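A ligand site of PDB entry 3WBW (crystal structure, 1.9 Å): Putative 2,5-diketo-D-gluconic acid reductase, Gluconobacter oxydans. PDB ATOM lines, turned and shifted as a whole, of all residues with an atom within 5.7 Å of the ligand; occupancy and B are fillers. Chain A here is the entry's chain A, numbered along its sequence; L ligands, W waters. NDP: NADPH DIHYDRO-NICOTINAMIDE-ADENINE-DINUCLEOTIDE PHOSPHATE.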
ATOM      1  N   GLY A  31       0.888   3.707 -25.718  1.00  0.00           N
ATOM      2  CA  GLY A  31       0.481   5.046 -26.126  1.00  0.00           C
ATOM      3  C   GLY A  31      -0.091   5.809 -24.940  1.00  0.00           C
ATOM      4  O   GLY A  31      -1.165   5.488 -24.433  1.00  0.00           O
ATOM      5  N   VAL A  32       0.643   6.798 -24.447  1.00  0.00           N
ATOM      6  CA  VAL A  32       0.103   7.617 -23.378  1.00  0.00           C
ATOM      7  C   VAL A  32      -0.720   8.673 -24.108  1.00  0.00           C
ATOM      8  O   VAL A  32      -0.350   9.082 -25.221  1.00  0.00           O
ATOM      9  CB  VAL A  32       1.244   8.190 -22.544  1.00  0.00           C
ATOM     10  CG1 VAL A  32       0.833   9.389 -21.712  1.00  0.00           C
ATOM     11  CG2 VAL A  32       1.835   7.077 -21.670  1.00  0.00           C
ATOM     12  N   TRP A  33      -1.871   9.043 -23.557  1.00  0.00           N
ATOM     13  CA  TRP A  33      -2.642  10.127 -24.193  1.00  0.00           C
ATOM     14  C   TRP A  33      -2.713  11.358 -23.288  1.00  0.00           C
ATOM     15  O   TRP A  33      -1.730  11.657 -22.609  1.00  0.00           O
ATOM     16  CB  TRP A  33      -4.036   9.696 -24.680  1.00  0.00           C
ATOM     17  CG  TRP A  33      -4.463  10.511 -25.949  1.00  0.00           C
ATOM     18  CD1 TRP A  33      -3.782  11.559 -26.552  1.00  0.00           C
ATOM     19  CD2 TRP A  33      -5.660  10.334 -26.731  1.00  0.00           C
ATOM     20  NE1 TRP A  33      -4.474  12.025 -27.652  1.00  0.00           N
ATOM     21  CE2 TRP A  33      -5.621  11.284 -27.798  1.00  0.00           C
ATOM     22  CE3 TRP A  33      -6.759   9.462 -26.644  1.00  0.00           C
ATOM     23  CZ2 TRP A  33      -6.636  11.394 -28.754  1.00  0.00           C
ATOM     24  CZ3 TRP A  33      -7.777   9.564 -27.611  1.00  0.00           C
ATOM     25  CH2 TRP A  33      -7.706  10.541 -28.645  1.00  0.00           C
ATOM     26  N   ASP A  56       5.279   5.833 -25.172  1.00  0.00           N
ATOM     27  CA  ASP A  56       5.249   6.908 -26.151  1.00  0.00           C
ATOM     28  C   ASP A  56       4.435   8.071 -25.636  1.00  0.00           C
ATOM     29  O   ASP A  56       3.294   7.906 -25.232  1.00  0.00           O
ATOM     30  CB  ASP A  56       4.740   6.360 -27.484  1.00  0.00           C
ATOM     31  CG  ASP A  56       4.558   7.429 -28.544  1.00  0.00           C
ATOM     32  OD1 ASP A  56       3.448   8.035 -28.567  1.00  0.00           O
ATOM     33  OD2 ASP A  56       5.468   7.608 -29.404  1.00  0.00           O
ATOM     34  N   TYR A  61       0.798  16.706 -24.809  1.00  0.00           N
ATOM     35  CA  TYR A  61       0.006  16.113 -23.706  1.00  0.00           C
ATOM     36  C   TYR A  61       0.331  16.721 -22.343  1.00  0.00           C
ATOM     37  O   TYR A  61      -0.420  16.543 -21.392  1.00  0.00           O
ATOM     38  CB  TYR A  61       0.094  14.573 -23.702  1.00  0.00           C
ATOM     39  CG  TYR A  61      -0.241  13.969 -25.045  1.00  0.00           C
ATOM     40  CD1 TYR A  61      -1.181  14.578 -25.879  1.00  0.00           C
ATOM     41  CD2 TYR A  61       0.407  12.811 -25.490  1.00  0.00           C
ATOM     42  CE1 TYR A  61      -1.458  14.043 -27.137  1.00  0.00           C
ATOM     43  CE2 TYR A  61       0.129  12.276 -26.728  1.00  0.00           C
ATOM     44  CZ  TYR A  61      -0.799  12.890 -27.542  1.00  0.00           C
ATOM     45  OH  TYR A  61      -1.067  12.351 -28.789  1.00  0.00           O
ATOM     46  N   LYS A  82       7.790  13.791 -28.585  1.00  0.00           N
ATOM     47  CA  LYS A  82       7.542  14.493 -29.844  1.00  0.00           C
ATOM     48  C   LYS A  82       7.571  16.005 -29.620  1.00  0.00           C
ATOM     49  O   LYS A  82       7.062  16.473 -28.584  1.00  0.00           O
ATOM     50  CB  LYS A  82       6.174  14.110 -30.419  1.00  0.00           C
ATOM     51  CG  LYS A  82       5.960  12.566 -30.535  1.00  0.00           C
ATOM     52  CD  LYS A  82       4.703  12.207 -31.303  1.00  0.00           C
ATOM     53  CE  LYS A  82       4.400  10.724 -31.133  1.00  0.00           C
ATOM     54  NZ  LYS A  82       3.780  10.449 -29.784  1.00  0.00           N
ATOM     55  N   HIS A 115       6.266  16.137 -34.423  1.00  0.00           N
ATOM     56  CA  HIS A 115       4.869  15.614 -34.271  1.00  0.00           C
ATOM     57  C   HIS A 115       4.013  15.690 -35.558  1.00  0.00           C
ATOM     58  O   HIS A 115       3.243  14.743 -35.862  1.00  0.00           O
ATOM     59  CB  HIS A 115       4.180  16.355 -33.133  1.00  0.00           C
ATOM     60  CG  HIS A 115       3.002  15.617 -32.538  1.00  0.00           C
ATOM     61  ND1 HIS A 115       2.662  15.744 -31.205  1.00  0.00           N
ATOM     62  CD2 HIS A 115       2.072  14.795 -33.081  1.00  0.00           C
ATOM     63  CE1 HIS A 115       1.586  15.019 -30.945  1.00  0.00           C
ATOM     64  NE2 HIS A 115       1.218  14.420 -32.069  1.00  0.00           N
ATOM     65  N   TRP A 116       4.097  16.812 -36.268  1.00  0.00           N
ATOM     66  CA  TRP A 116       3.415  17.030 -37.572  1.00  0.00           C
ATOM     67  C   TRP A 116       4.354  17.802 -38.493  1.00  0.00           C
ATOM     68  O   TRP A 116       5.139  18.636 -38.019  1.00  0.00           O
ATOM     69  CB  TRP A 116       2.108  17.904 -37.425  1.00  0.00           C
ATOM     70  CG  TRP A 116       0.997  17.185 -36.705  1.00  0.00           C
ATOM     71  CD1 TRP A 116       0.775  17.160 -35.357  1.00  0.00           C
ATOM     72  CD2 TRP A 116      -0.001  16.352 -37.303  1.00  0.00           C
ATOM     73  NE1 TRP A 116      -0.322  16.344 -35.069  1.00  0.00           N
ATOM     74  CE2 TRP A 116      -0.815  15.848 -36.250  1.00  0.00           C
ATOM     75  CE3 TRP A 116      -0.310  15.977 -38.631  1.00  0.00           C
ATOM     76  CZ2 TRP A 116      -1.898  14.994 -36.493  1.00  0.00           C
ATOM     77  CZ3 TRP A 116      -1.371  15.102 -38.853  1.00  0.00           C
ATOM     78  CH2 TRP A 116      -2.162  14.630 -37.778  1.00  0.00           C
ATOM     79  N   SER A 146       6.660  12.025 -37.442  1.00  0.00           N
ATOM     80  CA  SER A 146       5.305  11.526 -37.247  1.00  0.00           C
ATOM     81  C   SER A 146       4.429  12.278 -38.255  1.00  0.00           C
ATOM     82  O   SER A 146       4.623  13.516 -38.466  1.00  0.00           O
ATOM     83  CB  SER A 146       4.861  11.728 -35.799  1.00  0.00           C
ATOM     84  OG  SER A 146       3.508  11.327 -35.632  1.00  0.00           O
ATOM     85  N   ASN A 147       3.529  11.535 -38.905  1.00  0.00           N
ATOM     86  CA  ASN A 147       2.525  12.111 -39.834  1.00  0.00           C
ATOM     87  C   ASN A 147       3.115  12.724 -41.080  1.00  0.00           C
ATOM     88  O   ASN A 147       2.492  13.577 -41.710  1.00  0.00           O
ATOM     89  CB  ASN A 147       1.670  13.186 -39.123  1.00  0.00           C
ATOM     90  CG  ASN A 147       0.931  12.598 -37.927  1.00  0.00           C
ATOM     91  OD1 ASN A 147       0.292  11.552 -38.043  1.00  0.00           O
ATOM     92  ND2 ASN A 147       1.047  13.253 -36.767  1.00  0.00           N
ATOM     93  N   GLN A 168       5.867   7.664 -37.635  1.00  0.00           N
ATOM     94  CA  GLN A 168       4.703   7.229 -36.855  1.00  0.00           C
ATOM     95  C   GLN A 168       3.424   7.848 -37.451  1.00  0.00           C
ATOM     96  O   GLN A 168       3.224   9.111 -37.476  1.00  0.00           O
ATOM     97  CB  GLN A 168       4.881   7.646 -35.385  1.00  0.00           C
ATOM     98  CG  GLN A 168       3.834   7.098 -34.458  1.00  0.00           C
ATOM     99  CD  GLN A 168       3.850   7.709 -33.045  1.00  0.00           C
ATOM    100  OE1 GLN A 168       2.923   8.381 -32.675  1.00  0.00           O
ATOM    101  NE2 GLN A 168       4.944   7.483 -32.266  1.00  0.00           N
ATOM    102  N   TRP A 194       0.058   4.676 -35.028  1.00  0.00           N
ATOM    103  CA  TRP A 194      -0.865   5.220 -34.028  1.00  0.00           C
ATOM    104  C   TRP A 194      -2.310   5.028 -34.436  1.00  0.00           C
ATOM    105  O   TRP A 194      -2.598   4.747 -35.611  1.00  0.00           O
ATOM    106  CB  TRP A 194      -0.519   6.695 -33.694  1.00  0.00           C
ATOM    107  CG  TRP A 194      -0.687   7.756 -34.693  1.00  0.00           C
ATOM    108  CD1 TRP A 194       0.300   8.335 -35.472  1.00  0.00           C
ATOM    109  CD2 TRP A 194      -1.876   8.549 -34.919  1.00  0.00           C
ATOM    110  NE1 TRP A 194      -0.234   9.373 -36.214  1.00  0.00           N
ATOM    111  CE2 TRP A 194      -1.550   9.541 -35.886  1.00  0.00           C
ATOM    112  CE3 TRP A 194      -3.173   8.514 -34.402  1.00  0.00           C
ATOM    113  CZ2 TRP A 194      -2.484  10.481 -36.344  1.00  0.00           C
ATOM    114  CZ3 TRP A 194      -4.112   9.468 -34.871  1.00  0.00           C
ATOM    115  CH2 TRP A 194      -3.771  10.420 -35.827  1.00  0.00           C
ATOM    116  N   ARG A 195      -3.197   5.162 -33.449  1.00  0.00           N
ATOM    117  CA  ARG A 195      -4.597   4.741 -33.576  1.00  0.00           C
ATOM    118  C   ARG A 195      -4.694   3.283 -34.104  1.00  0.00           C
ATOM    119  O   ARG A 195      -5.429   3.016 -35.037  1.00  0.00           O
ATOM    120  CB  ARG A 195      -5.340   5.727 -34.512  1.00  0.00           C
ATOM    121  CG  ARG A 195      -6.856   5.541 -34.603  1.00  0.00           C
ATOM    122  CD  ARG A 195      -7.606   6.873 -34.834  1.00  0.00           C
ATOM    123  NE  ARG A 195      -7.554   7.617 -33.587  1.00  0.00           N
ATOM    124  CZ  ARG A 195      -7.604   8.939 -33.472  1.00  0.00           C
ATOM    125  NH1 ARG A 195      -7.709   9.712 -34.560  1.00  0.00           N
ATOM    126  NH2 ARG A 195      -7.518   9.484 -32.266  1.00  0.00           N
ATOM    127  N   PRO A 196      -3.892   2.331 -33.544  1.00  0.00           N
ATOM    128  CA  PRO A 196      -3.859   1.020 -34.222  1.00  0.00           C
ATOM    129  C   PRO A 196      -5.163   0.220 -34.198  1.00  0.00           C
ATOM    130  O   PRO A 196      -5.328  -0.736 -34.974  1.00  0.00           O
ATOM    131  CB  PRO A 196      -2.747   0.271 -33.459  1.00  0.00           C
ATOM    132  CG  PRO A 196      -2.700   0.916 -32.134  1.00  0.00           C
ATOM    133  CD  PRO A 196      -2.967   2.363 -32.411  1.00  0.00           C
ATOM    134  N   LEU A 197      -6.079   0.622 -33.289  1.00  0.00           N
ATOM    135  CA  LEU A 197      -7.352  -0.043 -33.141  1.00  0.00           C
ATOM    136  C   LEU A 197      -8.475   0.771 -33.784  1.00  0.00           C
ATOM    137  O   LEU A 197      -9.648   0.454 -33.614  1.00  0.00           O
ATOM    138  CB  LEU A 197      -7.650  -0.292 -31.651  1.00  0.00           C
ATOM    139  CG  LEU A 197      -6.614  -1.138 -30.904  1.00  0.00           C
ATOM    140  CD1 LEU A 197      -7.059  -1.375 -29.433  1.00  0.00           C
ATOM    141  CD2 LEU A 197      -6.349  -2.475 -31.617  1.00  0.00           C
ATOM    142  N   GLY A 198      -8.109   1.833 -34.507  1.00  0.00           N
ATOM    143  CA  GLY A 198      -9.091   2.632 -35.241  1.00  0.00           C
ATOM    144  C   GLY A 198     -10.177   3.143 -34.332  1.00  0.00           C
ATOM    145  O   GLY A 198     -11.362   3.051 -34.671  1.00  0.00           O
ATOM    146  N   LYS A 199      -9.768   3.645 -33.166  1.00  0.00           N
ATOM    147  CA  LYS A 199     -10.670   4.144 -32.105  1.00  0.00           C
ATOM    148  C   LYS A 199     -11.508   3.061 -31.363  1.00  0.00           C
ATOM    149  O   LYS A 199     -12.285   3.380 -30.447  1.00  0.00           O
ATOM    150  CB  LYS A 199     -11.574   5.293 -32.618  1.00  0.00           C
ATOM    151  CG  LYS A 199     -10.869   6.619 -32.794  1.00  0.00           C
ATOM    152  CD  LYS A 199     -11.889   7.733 -33.076  1.00  0.00           C
ATOM    153  CE  LYS A 199     -11.432   9.094 -32.516  1.00  0.00           C
ATOM    154  NZ  LYS A 199     -12.592   9.907 -31.978  1.00  0.00           N
ATOM    155  N   GLY A 200     -11.330   1.793 -31.750  1.00  0.00           N
ATOM    156  CA  GLY A 200     -12.027   0.664 -31.130  1.00  0.00           C
ATOM    157  C   GLY A 200     -13.159   0.132 -31.982  1.00  0.00           C
ATOM    158  O   GLY A 200     -13.841  -0.850 -31.630  1.00  0.00           O
ATOM    159  N   LEU A 203     -12.962  -3.396 -33.533  1.00  0.00           N
ATOM    160  CA  LEU A 203     -13.064  -4.446 -32.532  1.00  0.00           C
ATOM    161  C   LEU A 203     -14.404  -5.184 -32.549  1.00  0.00           C
ATOM    162  O   LEU A 203     -14.509  -6.278 -32.020  1.00  0.00           O
ATOM    163  CB  LEU A 203     -12.789  -3.895 -31.133  1.00  0.00           C
ATOM    164  CG  LEU A 203     -11.418  -3.197 -31.004  1.00  0.00           C
ATOM    165  CD1 LEU A 203     -11.170  -2.656 -29.597  1.00  0.00           C
ATOM    166  CD2 LEU A 203     -10.298  -4.106 -31.425  1.00  0.00           C
ATOM    167  N   THR A 218      -8.859 -12.199 -28.429  1.00  0.00           N
ATOM    168  CA  THR A 218      -9.782 -11.091 -28.554  1.00  0.00           C
ATOM    169  C   THR A 218      -9.595 -10.383 -29.885  1.00  0.00           C
ATOM    170  O   THR A 218      -8.536 -10.554 -30.520  1.00  0.00           O
ATOM    171  CB  THR A 218      -9.646 -10.073 -27.388  1.00  0.00           C
ATOM    172  OG1 THR A 218      -8.390  -9.391 -27.487  1.00  0.00           O
ATOM    173  CG2 THR A 218      -9.749 -10.787 -26.032  1.00  0.00           C
ATOM    174  N   ALA A 220      -9.149  -7.266 -30.283  1.00  0.00           N
ATOM    175  CA  ALA A 220      -8.015  -6.400 -30.067  1.00  0.00           C
ATOM    176  C   ALA A 220      -6.685  -7.137 -30.321  1.00  0.00           C
ATOM    177  O   ALA A 220      -5.769  -6.575 -30.966  1.00  0.00           O
ATOM    178  CB  ALA A 220      -8.073  -5.779 -28.639  1.00  0.00           C
ATOM    179  N   ILE A 235       1.588   1.110 -30.940  1.00  0.00           N
ATOM    180  CA  ILE A 235       1.443   1.742 -29.618  1.00  0.00           C
ATOM    181  C   ILE A 235      -0.032   1.881 -29.241  1.00  0.00           C
ATOM    182  O   ILE A 235      -0.615   2.975 -29.273  1.00  0.00           O
ATOM    183  CB  ILE A 235       2.208   3.095 -29.509  1.00  0.00           C
ATOM    184  CG1 ILE A 235       1.984   3.950 -30.754  1.00  0.00           C
ATOM    185  CG2 ILE A 235       3.707   2.799 -29.255  1.00  0.00           C
ATOM    186  CD1 ILE A 235       2.357   5.486 -30.588  1.00  0.00           C
ATOM    187  N   PRO A 236      -0.655   0.762 -28.866  1.00  0.00           N
ATOM    188  CA  PRO A 236      -2.044   0.827 -28.464  1.00  0.00           C
ATOM    189  C   PRO A 236      -2.186   1.612 -27.150  1.00  0.00           C
ATOM    190  O   PRO A 236      -1.329   1.509 -26.263  1.00  0.00           O
ATOM    191  CB  PRO A 236      -2.422  -0.624 -28.259  1.00  0.00           C
ATOM    192  CG  PRO A 236      -1.138  -1.328 -28.025  1.00  0.00           C
ATOM    193  CD  PRO A 236      -0.112  -0.612 -28.810  1.00  0.00           C
ATOM    194  N   LYS A 237      -3.278   2.347 -27.040  1.00  0.00           N
ATOM    195  CA  LYS A 237      -3.578   3.108 -25.826  1.00  0.00           C
ATOM    196  C   LYS A 237      -4.610   2.414 -24.971  1.00  0.00           C
ATOM    197  O   LYS A 237      -5.668   1.998 -25.466  1.00  0.00           O
ATOM    198  CB  LYS A 237      -4.133   4.459 -26.244  1.00  0.00           C
ATOM    199  CG  LYS A 237      -4.654   5.309 -25.073  1.00  0.00           C
ATOM    200  CD  LYS A 237      -6.149   5.211 -24.851  1.00  0.00           C
ATOM    201  CE  LYS A 237      -6.505   6.027 -23.580  1.00  0.00           C
ATOM    202  NZ  LYS A 237      -7.902   5.787 -23.123  1.00  0.00           N
ATOM    203  N   SER A 238      -4.327   2.308 -23.671  1.00  0.00           N
ATOM    204  CA  SER A 238      -5.340   1.864 -22.721  1.00  0.00           C
ATOM    205  C   SER A 238      -5.137   2.448 -21.326  1.00  0.00           C
ATOM    206  O   SER A 238      -4.004   2.658 -20.889  1.00  0.00           O
ATOM    207  CB  SER A 238      -5.398   0.330 -22.626  1.00  0.00           C
ATOM    208  OG  SER A 238      -6.519  -0.014 -21.852  1.00  0.00           O
ATOM    209  N   VAL A 239      -6.264   2.715 -20.674  1.00  0.00           N
ATOM    210  CA  VAL A 239      -6.312   3.203 -19.287  1.00  0.00           C
ATOM    211  C   VAL A 239      -6.693   2.039 -18.346  1.00  0.00           C
ATOM    212  O   VAL A 239      -6.480   2.132 -17.129  1.00  0.00           O
ATOM    213  CB  VAL A 239      -7.278   4.440 -19.182  1.00  0.00           C
ATOM    214  CG1 VAL A 239      -7.709   4.745 -17.723  1.00  0.00           C
ATOM    215  CG2 VAL A 239      -6.622   5.667 -19.854  1.00  0.00           C
ATOM    216  N   ASN A 240      -7.241   0.961 -18.928  1.00  0.00           N
ATOM    217  CA  ASN A 240      -7.678  -0.266 -18.242  1.00  0.00           C
ATOM    218  C   ASN A 240      -6.527  -1.270 -18.042  1.00  0.00           C
ATOM    219  O   ASN A 240      -6.054  -1.834 -19.021  1.00  0.00           O
ATOM    220  CB  ASN A 240      -8.672  -0.988 -19.169  1.00  0.00           C
ATOM    221  CG  ASN A 240     -10.105  -0.893 -18.720  1.00  0.00           C
ATOM    222  OD1 ASN A 240     -10.468  -1.391 -17.658  1.00  0.00           O
ATOM    223  ND2 ASN A 240     -10.962  -0.321 -19.569  1.00  0.00           N
ATOM    224  N   ARG A 243      -7.217  -4.393 -20.085  1.00  0.00           N
ATOM    225  CA  ARG A 243      -6.932  -4.239 -21.517  1.00  0.00           C
ATOM    226  C   ARG A 243      -5.459  -4.074 -21.780  1.00  0.00           C
ATOM    227  O   ARG A 243      -4.988  -4.503 -22.808  1.00  0.00           O
ATOM    228  CB  ARG A 243      -7.731  -3.098 -22.174  1.00  0.00           C
ATOM    229  CG  ARG A 243      -9.256  -3.391 -22.197  1.00  0.00           C
ATOM    230  CD  ARG A 243     -10.054  -2.172 -22.653  1.00  0.00           C
ATOM    231  NE  ARG A 243     -11.461  -2.521 -22.860  1.00  0.00           N
ATOM    232  CZ  ARG A 243     -12.400  -1.688 -23.300  1.00  0.00           C
ATOM    233  NH1 ARG A 243     -12.101  -0.427 -23.613  1.00  0.00           N
ATOM    234  NH2 ARG A 243     -13.647  -2.112 -23.437  1.00  0.00           N
ATOM    235  N   GLU A 246      -4.144  -7.545 -21.733  1.00  0.00           N
ATOM    236  CA  GLU A 246      -4.647  -8.189 -22.948  1.00  0.00           C
ATOM    237  C   GLU A 246      -3.899  -7.789 -24.216  1.00  0.00           C
ATOM    238  O   GLU A 246      -3.568  -8.647 -25.019  1.00  0.00           O
ATOM    239  CB  GLU A 246      -6.142  -7.898 -23.121  1.00  0.00           C
ATOM    240  CG  GLU A 246      -6.750  -8.303 -24.459  1.00  0.00           C
ATOM    241  CD  GLU A 246      -8.239  -8.008 -24.532  1.00  0.00           C
ATOM    242  OE1 GLU A 246      -8.948  -8.283 -23.529  1.00  0.00           O
ATOM    243  OE2 GLU A 246      -8.701  -7.515 -25.597  1.00  0.00           O
ATOM    244  N   ASN A 247      -3.612  -6.485 -24.380  1.00  0.00           N
ATOM    245  CA  ASN A 247      -2.993  -5.975 -25.605  1.00  0.00           C
ATOM    246  C   ASN A 247      -1.584  -6.507 -25.802  1.00  0.00           C
ATOM    247  O   ASN A 247      -1.063  -6.593 -26.932  1.00  0.00           O
ATOM    248  CB  ASN A 247      -2.994  -4.439 -25.624  1.00  0.00           C
ATOM    249  CG  ASN A 247      -4.389  -3.838 -25.866  1.00  0.00           C
ATOM    250  OD1 ASN A 247      -5.310  -4.564 -26.207  1.00  0.00           O
ATOM    251  ND2 ASN A 247      -4.535  -2.544 -25.647  1.00  0.00           N
HETATM  252  PA  NDP L   1      -6.196   3.130 -30.255  1.00  0.00           P
HETATM  253  O1A NDP L   1      -6.497   2.811 -31.672  1.00  0.00           O
HETATM  254  O2A NDP L   1      -5.036   2.514 -29.487  1.00  0.00           O
HETATM  255  O5B NDP L   1      -7.573   2.856 -29.456  1.00  0.00           O
HETATM  256  C5B NDP L   1      -7.604   3.094 -28.042  1.00  0.00           C
HETATM  257  C4B NDP L   1      -9.052   2.986 -27.576  1.00  0.00           C
HETATM  258  O4B NDP L   1      -9.475   1.621 -27.633  1.00  0.00           O
HETATM  259  C3B NDP L   1      -9.211   3.455 -26.147  1.00  0.00           C
HETATM  260  O3B NDP L   1     -10.499   4.093 -26.071  1.00  0.00           O
HETATM  261  C2B NDP L   1      -9.238   2.182 -25.315  1.00  0.00           C
HETATM  262  O2B NDP L   1     -10.064   2.357 -24.123  1.00  0.00           O
HETATM  263  C1B NDP L   1      -9.692   1.090 -26.302  1.00  0.00           C
HETATM  264  N9A NDP L   1      -8.985  -0.220 -26.124  1.00  0.00           N
HETATM  265  C8A NDP L   1      -7.640  -0.409 -25.979  1.00  0.00           C
HETATM  266  N7A NDP L   1      -7.352  -1.728 -25.829  1.00  0.00           N
HETATM  267  C5A NDP L   1      -8.540  -2.401 -25.885  1.00  0.00           C
HETATM  268  C6A NDP L   1      -8.902  -3.756 -25.788  1.00  0.00           C
HETATM  269  N6A NDP L   1      -7.990  -4.731 -25.582  1.00  0.00           N
HETATM  270  N1A NDP L   1     -10.209  -4.112 -25.867  1.00  0.00           N
HETATM  271  C2A NDP L   1     -11.170  -3.171 -26.057  1.00  0.00           C
HETATM  272  N3A NDP L   1     -10.861  -1.858 -26.139  1.00  0.00           N
HETATM  273  C4A NDP L   1      -9.551  -1.449 -26.068  1.00  0.00           C
HETATM  274  O3  NDP L   1      -5.892   4.694 -30.013  1.00  0.00           O
HETATM  275  PN  NDP L   1      -6.908   5.943 -29.901  1.00  0.00           P
HETATM  276  O1N NDP L   1      -7.734   5.906 -28.642  1.00  0.00           O
HETATM  277  O2N NDP L   1      -7.641   6.118 -31.209  1.00  0.00           O
HETATM  278  O5D NDP L   1      -5.734   7.051 -29.639  1.00  0.00           O
HETATM  279  C5D NDP L   1      -4.513   7.130 -30.390  1.00  0.00           C
HETATM  280  C4D NDP L   1      -3.208   6.758 -29.669  1.00  0.00           C
HETATM  281  O4D NDP L   1      -2.152   6.953 -30.640  1.00  0.00           O
HETATM  282  C3D NDP L   1      -2.767   7.582 -28.436  1.00  0.00           C
HETATM  283  O3D NDP L   1      -2.248   6.716 -27.442  1.00  0.00           O
HETATM  284  C2D NDP L   1      -1.603   8.483 -28.849  1.00  0.00           C
HETATM  285  O2D NDP L   1      -0.413   8.279 -28.053  1.00  0.00           O
HETATM  286  C1D NDP L   1      -1.334   8.108 -30.310  1.00  0.00           C
HETATM  287  N1N NDP L   1      -1.623   9.260 -31.174  1.00  0.00           N
HETATM  288  C2N NDP L   1      -0.628   9.791 -31.904  1.00  0.00           C
HETATM  289  C3N NDP L   1      -0.895  10.899 -32.727  1.00  0.00           C
HETATM  290  C7N NDP L   1       0.174  11.532 -33.571  1.00  0.00           C
HETATM  291  O7N NDP L   1      -0.141  12.563 -34.148  1.00  0.00           O
HETATM  292  N7N NDP L   1       1.393  10.959 -33.660  1.00  0.00           N
HETATM  293  C4N NDP L   1      -2.193  11.448 -32.784  1.00  0.00           C
HETATM  294  C5N NDP L   1      -3.197  10.876 -32.015  1.00  0.00           C
HETATM  295  C6N NDP L   1      -2.867   9.785 -31.218  1.00  0.00           C
HETATM  296  P2B NDP L   1      -9.372   2.281 -22.656  1.00  0.00           P
HETATM  297  O1X NDP L   1     -10.441   2.626 -21.628  1.00  0.00           O
HETATM  298  O2X NDP L   1      -8.273   3.290 -22.621  1.00  0.00           O
HETATM  299  O3X NDP L   1      -8.918   0.835 -22.557  1.00  0.00           O
HETATM  300  O   HOH W   1     -10.108   6.374 -27.627  1.00  0.00           O
HETATM  301  O   HOH W   2       1.199  11.536 -30.047  1.00  0.00           O
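Water W2 lies within hydrogen-bond range of the side-chain hydroxyl of Tyr 61 (2.7 Å) and the side-chain amino group of Lys 82 (2.8 Å).
NE1 of Trp 194 sits close to N7N of the ligand (3.4 Å).
The backbone nitrogen of Pro 196 sits close to an oxygen (O1A) of the ligand, at 3.2 Å.
Trp 33 touches the ligand (CZ3 to O1N, 3.8 Å).
OD1 of Asp 56 touches O2D of the ligand, at 3.9 Å.
Tyr 61 touches the ligand (OH to C2D, 3.9 Å).
CE of Lys 82 touches N7N of the ligand, at 3.9 Å.
CZ2 of Trp 116 touches O7N of the ligand (3.8 Å).
CG of Lys 199 touches O2N of the ligand (3.6 Å).
CD1 of Leu 203 touches N3A of the ligand (3.6 Å).
Ala 220 touches the ligand (CB to N6A, 3.2 Å).
CA of Pro 236 touches O2A of the ligand (3.6 Å).
Asn 240 touches the ligand.
Within 4 Å of the ligand: Gly 31, Val 32, Trp 33, Asp 56, Tyr 61, Lys 82, His 115, Trp 116, Ser 146, Asn 147, Gln 168, Trp 194, Arg 195, Pro 196, Leu 197, Gly 198, Lys 199, Leu 203, Ala 220, Pro 236, Lys 237, Ser 238, Val 239, Asn 240, Arg 243, Glu 246 and Asn 247.
N of Lys 237 sits at hydrogen-bond distance from O2A of the ligand (3.0 Å).
O2X of the ligand lies within salt-bridge range of NZ of Lys 237.
The side-chain hydroxyl of Ser 238 sits at hydrogen-bond distance from an oxygen (O3X) of the ligand (2.6 Å).
N of Leu 197 lies within hydrogen-bond range of O1A of the ligand (2.8 Å).
OD1 of Asn 247 sits at hydrogen-bond distance from N6A of the ligand.
O4D of the ligand lies within hydrogen-bond range of N of Arg 195, 3.5 Å away.
The guanidinium group of Arg 195 is in salt-bridge range of an oxygen (O2N) of the ligand (2.8 Å).
An oxygen (O2X) of the ligand is in hydrogen-bond range of the backbone NH of Val 239 (2.9 Å).
A nitrogen (N6A) of the ligand is in hydrogen-bond range of the side-chain carboxylate (OE2) of Glu 246 (2.9 Å).
The side-chain hydroxyl (OG) of Ser 146 is in hydrogen-bond range of a nitrogen (N7N) of the ligand (2.9 Å).
An oxygen (O2D) of the ligand sits at hydrogen-bond distance from the backbone carbonyl oxygen (O) of Val 32, at 2.9 Å.
An oxygen (O7N) of the ligand lies within hydrogen-bond range of the side-chain amide nitrogen of Asn 147.
A ring nitrogen (NE2) of His 115 lies within hydrogen-bond range of an oxygen (O7N) of the ligand.
OE1 of Gln 168 sits at hydrogen-bond distance from N7N of the ligand, 3.2 Å away.
O3X of the ligand lies within salt-bridge range of NH1 of Arg 243 (3.6 Å).
The backbone NH of Gly 198 sits at hydrogen-bond distance from an oxygen (O1A) of the ligand, at 3.4 Å.
O3D of the ligand sits at hydrogen-bond distance from O of Gly 31 (3.4 Å).
The backbone carbonyl oxygen (O) of Arg 243 sits close to the side-chain amide oxygen (OD1) of Asn 247 (3.4 Å).
The backbone carbonyl oxygen (O) of His 115 sits close to the side-chain hydroxyl (OG) of Ser 146 (3.4 Å).
OG of Ser 146 is in hydrogen-bond range of O of Gln 168 (2.9 Å).
The side-chain amide nitrogen (ND2) of Asn 147 lies within hydrogen-bond range of the backbone carbonyl oxygen (O) of His 115 (2.8 Å).
The indole nitrogen (NE1) of Trp 194 lies within hydrogen-bond range of the side-chain amide oxygen (OD1) of Asn 147.
The side-chain amide nitrogen (NE2) of Gln 168 lies within hydrogen-bond range of the side-chain carboxylate (OD2) of Asp 56 (2.9 Å).
The backbone NH (N) of Gly 31 is in hydrogen-bond range of the backbone carbonyl oxygen (O) of Pro 236, at 3.2 Å.
OD1 of Asp 56 is in salt-bridge range of NZ of Lys 82 (2.7 Å).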
